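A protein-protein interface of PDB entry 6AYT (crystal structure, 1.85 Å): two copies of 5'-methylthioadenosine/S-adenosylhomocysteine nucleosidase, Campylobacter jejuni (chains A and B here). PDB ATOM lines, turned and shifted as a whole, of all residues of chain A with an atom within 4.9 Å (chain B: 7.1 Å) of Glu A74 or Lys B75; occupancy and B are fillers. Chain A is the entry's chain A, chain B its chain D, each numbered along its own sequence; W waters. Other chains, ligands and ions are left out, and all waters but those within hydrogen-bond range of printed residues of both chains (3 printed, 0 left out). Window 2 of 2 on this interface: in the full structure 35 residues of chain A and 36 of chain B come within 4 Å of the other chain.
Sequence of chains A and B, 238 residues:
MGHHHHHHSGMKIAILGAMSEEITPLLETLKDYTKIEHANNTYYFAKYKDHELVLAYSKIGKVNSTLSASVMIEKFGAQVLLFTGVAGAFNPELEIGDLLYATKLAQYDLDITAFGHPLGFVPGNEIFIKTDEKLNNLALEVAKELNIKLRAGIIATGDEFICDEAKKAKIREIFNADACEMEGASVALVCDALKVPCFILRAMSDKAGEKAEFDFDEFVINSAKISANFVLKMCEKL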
ATOM      1  N   SER A  70       6.532  -3.647 -13.037  1.00  0.00           N
ATOM      2  CA  SER A  70       6.821  -4.883 -12.300  1.00  0.00           C
ATOM      3  C   SER A  70       8.276  -5.321 -12.487  1.00  0.00           C
ATOM      4  O   SER A  70       8.976  -5.624 -11.519  1.00  0.00           O
ATOM      5  CB  SER A  70       5.878  -6.002 -12.766  1.00  0.00           C
ATOM      6  OG  SER A  70       6.080  -7.197 -12.050  1.00  0.00           O
ATOM      7  N   VAL A  71       8.715  -5.354 -13.740  1.00  0.00           N
ATOM      8  CA  VAL A  71      10.086  -5.732 -14.096  1.00  0.00           C
ATOM      9  C   VAL A  71      11.123  -4.769 -13.509  1.00  0.00           C
ATOM     10  O   VAL A  71      12.148  -5.206 -12.965  1.00  0.00           O
ATOM     11  CB  VAL A  71      10.216  -5.834 -15.640  1.00  0.00           C
ATOM     12  CG1 VAL A  71      11.662  -5.776 -16.109  1.00  0.00           C
ATOM     13  CG2 VAL A  71       9.533  -7.111 -16.110  1.00  0.00           C
ATOM     14  N   MET A  72      10.867  -3.467 -13.610  1.00  0.00           N
ATOM     15  CA  MET A  72      11.836  -2.462 -13.144  1.00  0.00           C
ATOM     16  C   MET A  72      12.058  -2.537 -11.634  1.00  0.00           C
ATOM     17  O   MET A  72      13.178  -2.298 -11.163  1.00  0.00           O
ATOM     18  CB  MET A  72      11.405  -1.050 -13.569  1.00  0.00           C
ATOM     19  CG  MET A  72      11.545  -0.811 -15.064  1.00  0.00           C
ATOM     20  SD  MET A  72      10.658   0.647 -15.644  1.00  0.00           S
ATOM     21  CE  MET A  72      12.014   1.777 -15.959  1.00  0.00           C
ATOM     22  N   ILE A  73      11.005  -2.884 -10.892  1.00  0.00           N
ATOM     23  CA  ILE A  73      11.075  -3.028  -9.445  1.00  0.00           C
ATOM     24  C   ILE A  73      11.663  -4.390  -9.071  1.00  0.00           C
ATOM     25  O   ILE A  73      12.661  -4.452  -8.350  1.00  0.00           O
ATOM     26  CB  ILE A  73       9.695  -2.807  -8.788  1.00  0.00           C
ATOM     27  CG1 ILE A  73       9.258  -1.348  -9.012  1.00  0.00           C
ATOM     28  CG2 ILE A  73       9.724  -3.150  -7.296  1.00  0.00           C
ATOM     29  CD1 ILE A  73       7.797  -1.073  -8.726  1.00  0.00           C
ATOM     30  N   GLU A  74      11.065  -5.469  -9.570  1.00  0.00           N
ATOM     31  CA  GLU A  74      11.455  -6.815  -9.162  1.00  0.00           C
ATOM     32  C   GLU A  74      12.815  -7.246  -9.719  1.00  0.00           C
ATOM     33  O   GLU A  74      13.689  -7.691  -8.969  1.00  0.00           O
ATOM     34  CB  GLU A  74      10.374  -7.849  -9.525  1.00  0.00           C
ATOM     35  CG  GLU A  74      10.678  -9.321  -9.159  1.00  0.00           C
ATOM     36  CD  GLU A  74      10.810  -9.622  -7.655  1.00  0.00           C
ATOM     37  OE1 GLU A  74      10.210  -8.898  -6.827  1.00  0.00           O
ATOM     38  OE2 GLU A  74      11.552 -10.572  -7.314  1.00  0.00           O
ATOM     39  N   LYS A  75      12.980  -7.127 -11.029  1.00  0.00           N
ATOM     40  CA  LYS A  75      14.215  -7.553 -11.680  1.00  0.00           C
ATOM     41  C   LYS A  75      15.353  -6.546 -11.543  1.00  0.00           C
ATOM     42  O   LYS A  75      16.477  -6.940 -11.257  1.00  0.00           O
ATOM     43  CB  LYS A  75      13.990  -7.907 -13.158  1.00  0.00           C
ATOM     44  CG  LYS A  75      15.258  -8.326 -13.886  1.00  0.00           C
ATOM     45  CD  LYS A  75      15.202  -9.593 -14.727  1.00  0.00           C
ATOM     46  CE  LYS A  75      16.468  -9.682 -15.569  1.00  0.00           C
ATOM     47  NZ  LYS A  75      17.188 -10.934 -15.199  1.00  0.00           N
ATOM     48  N   PHE A  76      15.067  -5.259 -11.746  1.00  0.00           N
ATOM     49  CA  PHE A  76      16.119  -4.235 -11.764  1.00  0.00           C
ATOM     50  C   PHE A  76      16.198  -3.377 -10.498  1.00  0.00           C
ATOM     51  O   PHE A  76      16.935  -2.382 -10.474  1.00  0.00           O
ATOM     52  CB  PHE A  76      15.994  -3.378 -13.033  1.00  0.00           C
ATOM     53  CG  PHE A  76      16.057  -4.181 -14.306  1.00  0.00           C
ATOM     54  CD1 PHE A  76      17.129  -5.041 -14.551  1.00  0.00           C
ATOM     55  CD2 PHE A  76      15.049  -4.100 -15.253  1.00  0.00           C
ATOM     56  CE1 PHE A  76      17.189  -5.796 -15.714  1.00  0.00           C
ATOM     57  CE2 PHE A  76      15.108  -4.864 -16.410  1.00  0.00           C
ATOM     58  CZ  PHE A  76      16.181  -5.695 -16.654  1.00  0.00           C
ATOM     59  N   GLY A  77      15.466  -3.760  -9.453  1.00  0.00           N
ATOM     60  CA  GLY A  77      15.679  -3.214  -8.111  1.00  0.00           C
ATOM     61  C   GLY A  77      15.289  -1.777  -7.855  1.00  0.00           C
ATOM     62  O   GLY A  77      15.753  -1.183  -6.888  1.00  0.00           O
ATOM     63  N   LYS B  12       8.989 -25.964 -11.380  1.00  0.00           N
ATOM     64  CA  LYS B  12       8.174 -24.976 -10.690  1.00  0.00           C
ATOM     65  C   LYS B  12       7.013 -24.576 -11.590  1.00  0.00           C
ATOM     66  O   LYS B  12       7.237 -23.994 -12.650  1.00  0.00           O
ATOM     67  CB  LYS B  12       9.000 -23.736 -10.321  1.00  0.00           C
ATOM     68  CG  LYS B  12       8.438 -22.978  -9.129  1.00  0.00           C
ATOM     69  CD  LYS B  12       9.521 -22.208  -8.384  1.00  0.00           C
ATOM     70  CE  LYS B  12      10.480 -23.072  -7.596  1.00  0.00           C
ATOM     71  NZ  LYS B  12      11.825 -22.435  -7.479  1.00  0.00           N
ATOM     72  N   ILE B  36       2.746 -16.889   1.285  1.00  0.00           N
ATOM     73  CA  ILE B  36       3.566 -15.677   1.350  1.00  0.00           C
ATOM     74  C   ILE B  36       2.715 -14.491   0.911  1.00  0.00           C
ATOM     75  O   ILE B  36       2.036 -14.553  -0.121  1.00  0.00           O
ATOM     76  CB  ILE B  36       4.832 -15.759   0.461  1.00  0.00           C
ATOM     77  CG1 ILE B  36       5.702 -16.957   0.871  1.00  0.00           C
ATOM     78  CG2 ILE B  36       5.629 -14.454   0.552  1.00  0.00           C
ATOM     79  CD1 ILE B  36       6.901 -17.196  -0.016  1.00  0.00           C
ATOM     80  N   GLU B  37       2.739 -13.422   1.704  1.00  0.00           N
ATOM     81  CA  GLU B  37       2.084 -12.173   1.338  1.00  0.00           C
ATOM     82  C   GLU B  37       3.062 -11.358   0.491  1.00  0.00           C
ATOM     83  O   GLU B  37       4.167 -11.057   0.943  1.00  0.00           O
ATOM     84  CB  GLU B  37       1.683 -11.387   2.572  1.00  0.00           C
ATOM     85  CG  GLU B  37       0.703 -12.121   3.452  1.00  0.00           C
ATOM     86  CD  GLU B  37       0.036 -11.157   4.378  1.00  0.00           C
ATOM     87  OE1 GLU B  37      -1.201 -11.193   4.474  1.00  0.00           O
ATOM     88  OE2 GLU B  37       0.747 -10.329   4.990  1.00  0.00           O
ATOM     89  N   HIS B  38       2.653 -11.030  -0.734  1.00  0.00           N
ATOM     90  CA  HIS B  38       3.459 -10.197  -1.638  1.00  0.00           C
ATOM     91  C   HIS B  38       2.567  -9.529  -2.685  1.00  0.00           C
ATOM     92  O   HIS B  38       1.557 -10.102  -3.091  1.00  0.00           O
ATOM     93  CB  HIS B  38       4.527 -11.039  -2.343  1.00  0.00           C
ATOM     94  CG  HIS B  38       5.493 -10.233  -3.151  1.00  0.00           C
ATOM     95  ND1 HIS B  38       6.413  -9.379  -2.577  1.00  0.00           N
ATOM     96  CD2 HIS B  38       5.689 -10.152  -4.487  1.00  0.00           C
ATOM     97  CE1 HIS B  38       7.149  -8.825  -3.525  1.00  0.00           C
ATOM     98  NE2 HIS B  38       6.724  -9.269  -4.695  1.00  0.00           N
ATOM     99  N   ALA B  39       2.942  -8.316  -3.102  1.00  0.00           N
ATOM    100  CA  ALA B  39       2.227  -7.587  -4.165  1.00  0.00           C
ATOM    101  C   ALA B  39       0.741  -7.409  -3.837  1.00  0.00           C
ATOM    102  O   ALA B  39      -0.128  -7.550  -4.709  1.00  0.00           O
ATOM    103  CB  ALA B  39       2.412  -8.275  -5.519  1.00  0.00           C
ATOM    104  N   ALA B  69       1.085 -12.714 -12.811  1.00  0.00           N
ATOM    105  CA  ALA B  69       1.903 -13.517 -13.718  1.00  0.00           C
ATOM    106  C   ALA B  69       3.380 -13.102 -13.656  1.00  0.00           C
ATOM    107  O   ALA B  69       4.270 -13.960 -13.615  1.00  0.00           O
ATOM    108  CB  ALA B  69       1.383 -13.423 -15.141  1.00  0.00           C
ATOM    109  N   SER B  70       3.618 -11.789 -13.638  1.00  0.00           N
ATOM    110  CA  SER B  70       4.965 -11.225 -13.531  1.00  0.00           C
ATOM    111  C   SER B  70       5.664 -11.666 -12.245  1.00  0.00           C
ATOM    112  O   SER B  70       6.807 -12.119 -12.271  1.00  0.00           O
ATOM    113  CB  SER B  70       4.901  -9.695 -13.599  1.00  0.00           C
ATOM    114  OG  SER B  70       6.204  -9.139 -13.610  1.00  0.00           O
ATOM    115  N   VAL B  71       4.961 -11.515 -11.129  1.00  0.00           N
ATOM    116  CA  VAL B  71       5.469 -11.911  -9.808  1.00  0.00           C
ATOM    117  C   VAL B  71       5.769 -13.420  -9.721  1.00  0.00           C
ATOM    118  O   VAL B  71       6.829 -13.824  -9.214  1.00  0.00           O
ATOM    119  CB  VAL B  71       4.476 -11.467  -8.713  1.00  0.00           C
ATOM    120  CG1 VAL B  71       4.701 -12.194  -7.391  1.00  0.00           C
ATOM    121  CG2 VAL B  71       4.548  -9.958  -8.517  1.00  0.00           C
ATOM    122  N   MET B  72       4.849 -14.246 -10.222  1.00  0.00           N
ATOM    123  CA  MET B  72       5.004 -15.700 -10.124  1.00  0.00           C
ATOM    124  C   MET B  72       6.229 -16.216 -10.901  1.00  0.00           C
ATOM    125  O   MET B  72       6.891 -17.174 -10.471  1.00  0.00           O
ATOM    126  CB  MET B  72       3.729 -16.417 -10.585  1.00  0.00           C
ATOM    127  CG  MET B  72       2.566 -16.252  -9.630  1.00  0.00           C
ATOM    128  SD  MET B  72       0.972 -16.685 -10.326  1.00  0.00           S
ATOM    129  CE  MET B  72       0.651 -18.238  -9.502  1.00  0.00           C
ATOM    130  N   ILE B  73       6.531 -15.560 -12.021  1.00  0.00           N
ATOM    131  CA  ILE B  73       7.683 -15.907 -12.844  1.00  0.00           C
ATOM    132  C   ILE B  73       8.961 -15.295 -12.267  1.00  0.00           C
ATOM    133  O   ILE B  73       9.915 -16.021 -11.988  1.00  0.00           O
ATOM    134  CB  ILE B  73       7.471 -15.486 -14.315  1.00  0.00           C
ATOM    135  CG1 ILE B  73       6.308 -16.292 -14.912  1.00  0.00           C
ATOM    136  CG2 ILE B  73       8.755 -15.677 -15.133  1.00  0.00           C
ATOM    137  CD1 ILE B  73       5.783 -15.754 -16.218  1.00  0.00           C
ATOM    138  N   GLU B  74       8.968 -13.976 -12.069  1.00  0.00           N
ATOM    139  CA  GLU B  74      10.185 -13.260 -11.676  1.00  0.00           C
ATOM    140  C   GLU B  74      10.580 -13.537 -10.220  1.00  0.00           C
ATOM    141  O   GLU B  74      11.734 -13.901  -9.952  1.00  0.00           O
ATOM    142  CB  GLU B  74      10.035 -11.748 -11.887  1.00  0.00           C
ATOM    143  CG  GLU B  74       9.789 -11.349 -13.331  1.00  0.00           C
ATOM    144  CD  GLU B  74      11.056 -11.244 -14.143  1.00  0.00           C
ATOM    145  OE1 GLU B  74      11.271 -10.161 -14.746  1.00  0.00           O
ATOM    146  OE2 GLU B  74      11.846 -12.216 -14.215  1.00  0.00           O
ATOM    147  N   LYS B  75       9.640 -13.366  -9.290  1.00  0.00           N
ATOM    148  CA  LYS B  75       9.931 -13.572  -7.877  1.00  0.00           C
ATOM    149  C   LYS B  75       9.936 -15.045  -7.472  1.00  0.00           C
ATOM    150  O   LYS B  75      10.837 -15.477  -6.746  1.00  0.00           O
ATOM    151  CB  LYS B  75       8.976 -12.790  -6.970  1.00  0.00           C
ATOM    152  CG  LYS B  75       9.305 -12.968  -5.489  1.00  0.00           C
ATOM    153  CD  LYS B  75       8.654 -11.918  -4.638  1.00  0.00           C
ATOM    154  CE  LYS B  75       9.067 -12.000  -3.174  1.00  0.00           C
ATOM    155  NZ  LYS B  75      10.431 -11.474  -2.946  1.00  0.00           N
ATOM    156  N   PHE B  76       8.944 -15.810  -7.914  1.00  0.00           N
ATOM    157  CA  PHE B  76       8.775 -17.194  -7.437  1.00  0.00           C
ATOM    158  C   PHE B  76       9.223 -18.271  -8.434  1.00  0.00           C
ATOM    159  O   PHE B  76       8.989 -19.449  -8.204  1.00  0.00           O
ATOM    160  CB  PHE B  76       7.334 -17.415  -6.962  1.00  0.00           C
ATOM    161  CG  PHE B  76       6.909 -16.459  -5.878  1.00  0.00           C
ATOM    162  CD1 PHE B  76       7.650 -16.345  -4.713  1.00  0.00           C
ATOM    163  CD2 PHE B  76       5.769 -15.667  -6.022  1.00  0.00           C
ATOM    164  CE1 PHE B  76       7.273 -15.465  -3.710  1.00  0.00           C
ATOM    165  CE2 PHE B  76       5.385 -14.786  -5.024  1.00  0.00           C
ATOM    166  CZ  PHE B  76       6.144 -14.679  -3.867  1.00  0.00           C
ATOM    167  N   GLY B  77       9.882 -17.862  -9.517  1.00  0.00           N
ATOM    168  CA  GLY B  77      10.624 -18.773 -10.375  1.00  0.00           C
ATOM    169  C   GLY B  77       9.825 -19.739 -11.226  1.00  0.00           C
ATOM    170  O   GLY B  77      10.364 -20.761 -11.667  1.00  0.00           O
ATOM    171  N   ALA B  78       8.552 -19.429 -11.484  1.00  0.00           N
ATOM    172  CA  ALA B  78       7.718 -20.313 -12.281  1.00  0.00           C
ATOM    173  C   ALA B  78       8.344 -20.562 -13.655  1.00  0.00           C
ATOM    174  O   ALA B  78       8.775 -19.623 -14.332  1.00  0.00           O
ATOM    175  CB  ALA B  78       6.322 -19.734 -12.440  1.00  0.00           C
HETATM  176  O   HOH W   1      14.780 -13.088 -14.915  1.00  0.00           O
HETATM  177  O   HOH W   2       7.793  -8.544  -7.085  1.00  0.00           O
HETATM  178  O   HOH W   3       8.166  -8.968 -11.764  1.00  0.00           O
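OG of Ser A70 is in hydrogen-bond range of OG of Ser B70 (2.5 Å).
The backbone carbonyl oxygen of Val A71 sits at hydrogen-bond distance from the backbone NH of Phe A76 (3.2 Å).
Among the printed residues, pairs that only touch across the chains: Glu A74 with Lys B75, Glu A74 with Glu B74, Val A71 with Glu B74 and Lys A75 with Glu B74.
Of chain B, only Glu B74 (3.7 Å) and Lys B75 (3.4 Å) come within 4 Å of Glu A74. Lys B75 touches just one residue of chain A: Glu A74 (3.4 Å). Of the printed residues of chain B, Ser A70 touches Ser B70. Printed residues of chain B within 4 Å of Val A71: Glu B74 (3.8 Å). Printed residues of chain A within 4 Å of Ser B70: Ser A70 (2.5 Å). Of the printed residues of chain B, Lys A75 touches Glu B74. Ala B78 touches none of the printed residues of chain A. The nearest printed residue of chain A that does not touch Lys B75 is Lys A75 (7.3 Å).
Hydrophobic or aromatic side chains of chain A that line the printed part of chain B: Val A71. Of the 15 printed residues of chain B, 3 touch a printed residue of chain A. Printed residues of chain B that touch a printed residue of chain A: Ser B70, Glu B74 and Lys B75.
Ser A70 touches its own counterpart, Ser B70. Val A71 touches Glu B74, but with the chains exchanged Glu A74 does not touch Val B71 (5.9 Å). Glu B74 touches its own counterpart, Glu A74. Glu A74 touches Lys B75, and with the chains exchanged Lys A75 touches Glu B74. 8 positions are printed for both chains.
Water W2 lies within hydrogen-bond range of OE1 of Glu A74 (2.5 Å) and NE2 of His B38 (2.7 Å). Water W3 lies within hydrogen-bond range of OG of Ser B70 and OG of Ser A70. Water W1 lies within hydrogen-bond range of OE2 of Glu B74 (3.1 Å) and NZ of Lys A75 (3.2 Å).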
